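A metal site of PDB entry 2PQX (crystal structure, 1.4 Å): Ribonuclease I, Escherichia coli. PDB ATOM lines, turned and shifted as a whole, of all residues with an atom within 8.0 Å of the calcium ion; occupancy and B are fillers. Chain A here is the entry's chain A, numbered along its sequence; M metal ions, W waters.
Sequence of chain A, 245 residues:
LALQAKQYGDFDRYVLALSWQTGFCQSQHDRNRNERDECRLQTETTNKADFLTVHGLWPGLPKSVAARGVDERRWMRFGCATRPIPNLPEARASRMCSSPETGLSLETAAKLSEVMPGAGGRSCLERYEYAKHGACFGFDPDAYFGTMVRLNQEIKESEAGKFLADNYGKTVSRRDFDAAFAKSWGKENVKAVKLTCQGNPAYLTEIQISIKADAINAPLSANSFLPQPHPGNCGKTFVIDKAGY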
ATOM      1  N   TRP A  20     -25.480  19.394  34.282  1.00  0.00           N
ATOM      2  CA  TRP A  20     -25.518  18.327  33.300  1.00  0.00           C
ATOM      3  C   TRP A  20     -24.096  18.575  32.805  1.00  0.00           C
ATOM      4  O   TRP A  20     -23.859  19.434  31.949  1.00  0.00           O
ATOM      5  CB  TRP A  20     -26.556  18.602  32.213  1.00  0.00           C
ATOM      6  CG  TRP A  20     -26.599  17.508  31.195  1.00  0.00           C
ATOM      7  CD1 TRP A  20     -26.447  17.646  29.854  1.00  0.00           C
ATOM      8  CD2 TRP A  20     -26.725  16.110  31.447  1.00  0.00           C
ATOM      9  NE1 TRP A  20     -26.474  16.417  29.240  1.00  0.00           N
ATOM     10  CE2 TRP A  20     -26.648  15.453  30.197  1.00  0.00           C
ATOM     11  CE3 TRP A  20     -26.909  15.335  32.602  1.00  0.00           C
ATOM     12  CZ2 TRP A  20     -26.732  14.052  30.075  1.00  0.00           C
ATOM     13  CZ3 TRP A  20     -27.000  13.946  32.484  1.00  0.00           C
ATOM     14  CH2 TRP A  20     -26.909  13.327  31.220  1.00  0.00           C
ATOM     15  N   GLN A  21     -23.158  17.855  33.394  1.00  0.00           N
ATOM     16  CA  GLN A  21     -21.730  18.026  33.134  1.00  0.00           C
ATOM     17  C   GLN A  21     -21.283  18.134  31.692  1.00  0.00           C
ATOM     18  O   GLN A  21     -20.443  18.978  31.366  1.00  0.00           O
ATOM     19  CB  GLN A  21     -20.933  16.937  33.859  1.00  0.00           C
ATOM     20  CG  GLN A  21     -19.457  17.263  33.986  1.00  0.00           C
ATOM     21  CD  GLN A  21     -19.199  18.514  34.811  1.00  0.00           C
ATOM     22  OE1 GLN A  21     -18.055  18.981  34.913  1.00  0.00           O
ATOM     23  NE2 GLN A  21     -20.243  19.065  35.402  1.00  0.00           N
ATOM     24  N   THR A  22     -21.808  17.284  30.818  1.00  0.00           N
ATOM     25  CA  THR A  22     -21.442  17.348  29.415  1.00  0.00           C
ATOM     26  C   THR A  22     -21.837  18.715  28.857  1.00  0.00           C
ATOM     27  O   THR A  22     -21.059  19.360  28.144  1.00  0.00           O
ATOM     28  CB  THR A  22     -22.132  16.236  28.619  1.00  0.00           C
ATOM     29  OG1 THR A  22     -23.530  16.239  28.931  1.00  0.00           O
ATOM     30  CG2 THR A  22     -21.535  14.885  28.974  1.00  0.00           C
ATOM     31  N   GLY A  23     -23.040  19.162  29.194  1.00  0.00           N
ATOM     32  CA  GLY A  23     -23.519  20.457  28.729  1.00  0.00           C
ATOM     33  C   GLY A  23     -22.714  21.604  29.310  1.00  0.00           C
ATOM     34  O   GLY A  23     -22.448  22.598  28.624  1.00  0.00           O
ATOM     35  N   PHE A  24     -22.326  21.485  30.573  1.00  0.00           N
ATOM     36  CA  PHE A  24     -21.525  22.506  31.219  1.00  0.00           C
ATOM     37  C   PHE A  24     -20.235  22.658  30.423  1.00  0.00           C
ATOM     38  O   PHE A  24     -19.826  23.763  30.071  1.00  0.00           O
ATOM     39  CB  PHE A  24     -21.170  22.101  32.647  1.00  0.00           C
ATOM     40  CG  PHE A  24     -20.140  22.982  33.283  1.00  0.00           C
ATOM     41  CD1 PHE A  24     -20.446  24.286  33.640  1.00  0.00           C
ATOM     42  CD2 PHE A  24     -18.839  22.523  33.470  1.00  0.00           C
ATOM     43  CE1 PHE A  24     -19.469  25.133  34.169  1.00  0.00           C
ATOM     44  CE2 PHE A  24     -17.858  23.354  34.005  1.00  0.00           C
ATOM     45  CZ  PHE A  24     -18.173  24.657  34.347  1.00  0.00           C
ATOM     46  N   CYS A  25     -19.602  21.538  30.139  1.00  0.00           N
ATOM     47  CA  CYS A  25     -18.359  21.527  29.392  1.00  0.00           C
ATOM     48  C   CYS A  25     -18.540  22.082  27.984  1.00  0.00           C
ATOM     49  O   CYS A  25     -17.687  22.820  27.477  1.00  0.00           O
ATOM     50  CB  CYS A  25     -17.790  20.112  29.351  1.00  0.00           C
ATOM     51  SG  CYS A  25     -17.171  19.564  30.979  1.00  0.00           S
ATOM     52  N   GLN A  26     -19.651  21.735  27.348  1.00  0.00           N
ATOM     53  CA  GLN A  26     -19.946  22.219  26.004  1.00  0.00           C
ATOM     54  C   GLN A  26     -20.080  23.737  26.038  1.00  0.00           C
ATOM     55  O   GLN A  26     -19.556  24.438  25.178  1.00  0.00           O
ATOM     56  CB  GLN A  26     -21.261  21.603  25.501  1.00  0.00           C
ATOM     57  CG  GLN A  26     -21.618  21.929  24.047  1.00  0.00           C
ATOM     58  CD  GLN A  26     -20.685  21.252  23.069  1.00  0.00           C
ATOM     59  OE1 GLN A  26     -20.572  20.032  23.054  1.00  0.00           O
ATOM     60  NE2 GLN A  26     -20.020  22.039  22.236  1.00  0.00           N
ATOM     61  N   SER A  27     -20.786  24.242  27.047  1.00  0.00           N
ATOM     62  CA  SER A  27     -20.999  25.677  27.194  1.00  0.00           C
ATOM     63  C   SER A  27     -19.696  26.463  27.378  1.00  0.00           C
ATOM     64  O   SER A  27     -19.484  27.493  26.719  1.00  0.00           O
ATOM     65  CB  SER A  27     -21.935  25.944  28.377  1.00  0.00           C
ATOM     66  OG  SER A  27     -22.118  27.327  28.586  1.00  0.00           O
ATOM     67  N   HIS A  29     -16.829  25.622  26.466  1.00  0.00           N
ATOM     68  CA  HIS A  29     -16.174  25.531  25.162  1.00  0.00           C
ATOM     69  C   HIS A  29     -16.794  26.499  24.131  1.00  0.00           C
ATOM     70  O   HIS A  29     -16.070  27.209  23.435  1.00  0.00           O
ATOM     71  CB  HIS A  29     -16.263  24.097  24.618  1.00  0.00           C
ATOM     72  CG  HIS A  29     -15.727  23.941  23.234  1.00  0.00           C
ATOM     73  ND1 HIS A  29     -14.398  24.153  22.925  1.00  0.00           N
ATOM     74  CD2 HIS A  29     -16.345  23.668  22.062  1.00  0.00           C
ATOM     75  CE1 HIS A  29     -14.219  24.027  21.627  1.00  0.00           C
ATOM     76  NE2 HIS A  29     -15.387  23.722  21.076  1.00  0.00           N
ATOM     77  N   ASP A  30     -18.112  26.535  24.027  1.00  0.00           N
ATOM     78  CA  ASP A  30     -18.776  27.417  23.071  1.00  0.00           C
ATOM     79  C   ASP A  30     -18.566  28.899  23.372  1.00  0.00           C
ATOM     80  O   ASP A  30     -18.599  29.723  22.459  1.00  0.00           O
ATOM     81  CB  ASP A  30     -20.286  27.130  22.999  1.00  0.00           C
ATOM     82  CG  ASP A  30     -20.599  25.735  22.499  1.00  0.00           C
ATOM     83  OD1 ASP A  30     -19.677  25.031  22.023  1.00  0.00           O
ATOM     84  OD2 ASP A  30     -21.786  25.342  22.568  1.00  0.00           O
ATOM     85  N   GLN A  42     -13.040  14.654  31.066  1.00  0.00           N
ATOM     86  CA  GLN A  42     -14.377  14.076  30.947  1.00  0.00           C
ATOM     87  C   GLN A  42     -14.456  13.041  29.835  1.00  0.00           C
ATOM     88  O   GLN A  42     -14.081  13.302  28.693  1.00  0.00           O
ATOM     89  CB  GLN A  42     -15.399  15.182  30.684  1.00  0.00           C
ATOM     90  CG  GLN A  42     -16.818  14.688  30.493  1.00  0.00           C
ATOM     91  CD  GLN A  42     -17.806  15.803  30.241  1.00  0.00           C
ATOM     92  OE1 GLN A  42     -17.706  16.528  29.247  1.00  0.00           O
ATOM     93  NE2 GLN A  42     -18.776  15.951  31.138  1.00  0.00           N
ATOM     94  N   TYR A 168     -30.155  10.466  26.194  1.00  0.00           N
ATOM     95  CA  TYR A 168     -28.801  10.960  26.043  1.00  0.00           C
ATOM     96  C   TYR A 168     -28.488  11.300  24.585  1.00  0.00           C
ATOM     97  O   TYR A 168     -28.582  10.442  23.698  1.00  0.00           O
ATOM     98  CB  TYR A 168     -27.827   9.905  26.566  1.00  0.00           C
ATOM     99  CG  TYR A 168     -26.378  10.297  26.515  1.00  0.00           C
ATOM    100  CD1 TYR A 168     -25.477   9.654  25.668  1.00  0.00           C
ATOM    101  CD2 TYR A 168     -25.883  11.303  27.351  1.00  0.00           C
ATOM    102  CE1 TYR A 168     -24.142   9.994  25.644  1.00  0.00           C
ATOM    103  CE2 TYR A 168     -24.534  11.657  27.337  1.00  0.00           C
ATOM    104  CZ  TYR A 168     -23.671  10.993  26.483  1.00  0.00           C
ATOM    105  OH  TYR A 168     -22.336  11.333  26.459  1.00  0.00           O
ATOM    106  N   TYR A 203     -29.291  23.392  24.694  1.00  0.00           N
ATOM    107  CA  TYR A 203     -28.867  22.115  25.244  1.00  0.00           C
ATOM    108  C   TYR A 203     -28.733  22.317  26.740  1.00  0.00           C
ATOM    109  O   TYR A 203     -28.347  23.378  27.217  1.00  0.00           O
ATOM    110  CB  TYR A 203     -27.559  21.588  24.625  1.00  0.00           C
ATOM    111  CG  TYR A 203     -26.351  22.480  24.723  1.00  0.00           C
ATOM    112  CD1 TYR A 203     -25.996  23.325  23.675  1.00  0.00           C
ATOM    113  CD2 TYR A 203     -25.549  22.464  25.861  1.00  0.00           C
ATOM    114  CE1 TYR A 203     -24.865  24.135  23.751  1.00  0.00           C
ATOM    115  CE2 TYR A 203     -24.418  23.278  25.950  1.00  0.00           C
ATOM    116  CZ  TYR A 203     -24.078  24.109  24.893  1.00  0.00           C
ATOM    117  OH  TYR A 203     -22.963  24.905  24.981  1.00  0.00           O
ATOM    118  N   VAL A 239     -31.693  19.854  23.888  1.00  0.00           N
ATOM    119  CA  VAL A 239     -30.876  18.674  23.687  1.00  0.00           C
ATOM    120  C   VAL A 239     -30.161  18.229  24.958  1.00  0.00           C
ATOM    121  O   VAL A 239     -29.644  19.059  25.719  1.00  0.00           O
ATOM    122  CB  VAL A 239     -29.811  18.934  22.607  1.00  0.00           C
ATOM    123  CG1 VAL A 239     -28.974  17.678  22.386  1.00  0.00           C
ATOM    124  CG2 VAL A 239     -30.474  19.367  21.309  1.00  0.00           C
ATOM    125  N   ILE A 240     -30.139  16.924  25.175  1.00  0.00           N
ATOM    126  CA  ILE A 240     -29.440  16.363  26.320  1.00  0.00           C
ATOM    127  C   ILE A 240     -28.039  16.139  25.761  1.00  0.00           C
ATOM    128  O   ILE A 240     -27.724  15.072  25.212  1.00  0.00           O
ATOM    129  CB  ILE A 240     -30.060  15.024  26.764  1.00  0.00           C
ATOM    130  CG1 ILE A 240     -31.539  15.241  27.110  1.00  0.00           C
ATOM    131  CG2 ILE A 240     -29.297  14.441  27.938  1.00  0.00           C
ATOM    132  CD1 ILE A 240     -31.771  16.310  28.164  1.00  0.00           C
ATOM    133  N   ASP A 241     -27.210  17.168  25.866  1.00  0.00           N
ATOM    134  CA  ASP A 241     -25.855  17.137  25.340  1.00  0.00           C
ATOM    135  C   ASP A 241     -25.039  15.909  25.701  1.00  0.00           C
ATOM    136  O   ASP A 241     -25.040  15.470  26.849  1.00  0.00           O
ATOM    137  CB  ASP A 241     -25.101  18.386  25.797  1.00  0.00           C
ATOM    138  CG  ASP A 241     -23.711  18.476  25.200  1.00  0.00           C
ATOM    139  OD1 ASP A 241     -23.590  18.580  23.960  1.00  0.00           O
ATOM    140  OD2 ASP A 241     -22.725  18.440  25.967  1.00  0.00           O
ATOM    141  N   LYS A 242     -24.361  15.352  24.695  1.00  0.00           N
ATOM    142  CA  LYS A 242     -23.501  14.185  24.892  1.00  0.00           C
ATOM    143  C   LYS A 242     -22.063  14.617  25.126  1.00  0.00           C
ATOM    144  O   LYS A 242     -21.679  15.750  24.802  1.00  0.00           O
ATOM    145  CB  LYS A 242     -23.512  13.261  23.667  1.00  0.00           C
ATOM    146  CG  LYS A 242     -24.776  12.458  23.450  1.00  0.00           C
ATOM    147  CD  LYS A 242     -24.597  11.542  22.240  1.00  0.00           C
ATOM    148  CE  LYS A 242     -25.812  10.634  22.043  1.00  0.00           C
ATOM    149  NZ  LYS A 242     -25.641   9.730  20.860  1.00  0.00           N
ATOM    150  N   ALA A 243     -21.251  13.727  25.686  1.00  0.00           N
ATOM    151  CA  ALA A 243     -19.845  14.028  25.920  1.00  0.00           C
ATOM    152  C   ALA A 243     -19.200  14.321  24.575  1.00  0.00           C
ATOM    153  O   ALA A 243     -19.597  13.759  23.549  1.00  0.00           O
ATOM    154  CB  ALA A 243     -19.160  12.839  26.584  1.00  0.00           C
ATOM    155  N   GLY A 244     -18.216  15.211  24.574  1.00  0.00           N
ATOM    156  CA  GLY A 244     -17.556  15.574  23.333  1.00  0.00           C
ATOM    157  C   GLY A 244     -18.058  16.918  22.829  1.00  0.00           C
ATOM    158  O   GLY A 244     -19.234  17.241  22.991  1.00  0.00           O
ATOM    159  N   TYR A 245     -17.166  17.686  22.222  1.00  0.00           N
ATOM    160  CA  TYR A 245     -17.495  19.004  21.701  1.00  0.00           C
ATOM    161  C   TYR A 245     -18.001  18.940  20.270  1.00  0.00           C
ATOM    162  O   TYR A 245     -19.086  19.490  19.995  1.00  0.00           O
ATOM    163  CB  TYR A 245     -16.259  19.911  21.778  1.00  0.00           C
ATOM    164  CG  TYR A 245     -15.741  20.135  23.185  1.00  0.00           C
ATOM    165  CD1 TYR A 245     -14.461  20.632  23.400  1.00  0.00           C
ATOM    166  CD2 TYR A 245     -16.537  19.868  24.292  1.00  0.00           C
ATOM    167  CE1 TYR A 245     -13.985  20.856  24.695  1.00  0.00           C
ATOM    168  CE2 TYR A 245     -16.076  20.083  25.591  1.00  0.00           C
ATOM    169  CZ  TYR A 245     -14.795  20.571  25.780  1.00  0.00           C
ATOM    170  OH  TYR A 245     -14.323  20.782  27.057  1.00  0.00           O
ATOM    171  OXT TYR A 245     -17.295  18.351  19.424  1.00  0.00           O
HETATM  172 CA    CA M   1     -21.267  17.948  24.005  1.00  0.00          CA
HETATM  173  O   HOH W   1     -19.719  18.372  25.949  1.00  0.00           O
HETATM  174  O   HOH W   2     -22.090  17.103  21.859  1.00  0.00           O
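OE1 of Gln 26 sits close to O of Tyr 245 (3.4 Å).
The side-chain hydroxyl (OH) of Tyr 203 sits close to the backbone carbonyl oxygen (O) of Gln 26.
The side-chain carboxylate (OD1) of Asp 30 lies within hydrogen-bond range of the side-chain amide nitrogen (NE2) of Gln 26.
O of Asp 241 lies within hydrogen-bond range of OG1 of Thr 22, at 2.7 Å.
The side-chain carboxylate (OD2) of Asp 241 sits close to the backbone NH (N) of Gly 23, 3.3 Å away.
NE1 of Trp 20 lies within hydrogen-bond range of O of Asp 241 (2.9 Å).
Of the 20 residues printed, 4 come within 4 Å of the calcium ion.
The nearest printed residue that does not touch the calcium ion is Ala 243 (4.2 Å).
The calcium ion is bound by O of Lys 242 (2.4 Å), O of Gly 244 (2.4 Å), OE1 of Gln 26 (2.4 Å), OD1 of Asp 241 (2.4 Å), water W2 (2.4 Å), OD2 of Asp 241 (2.5 Å) and water W1 (2.5 Å).
The calcium ion has seven donor atoms within binding distance.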
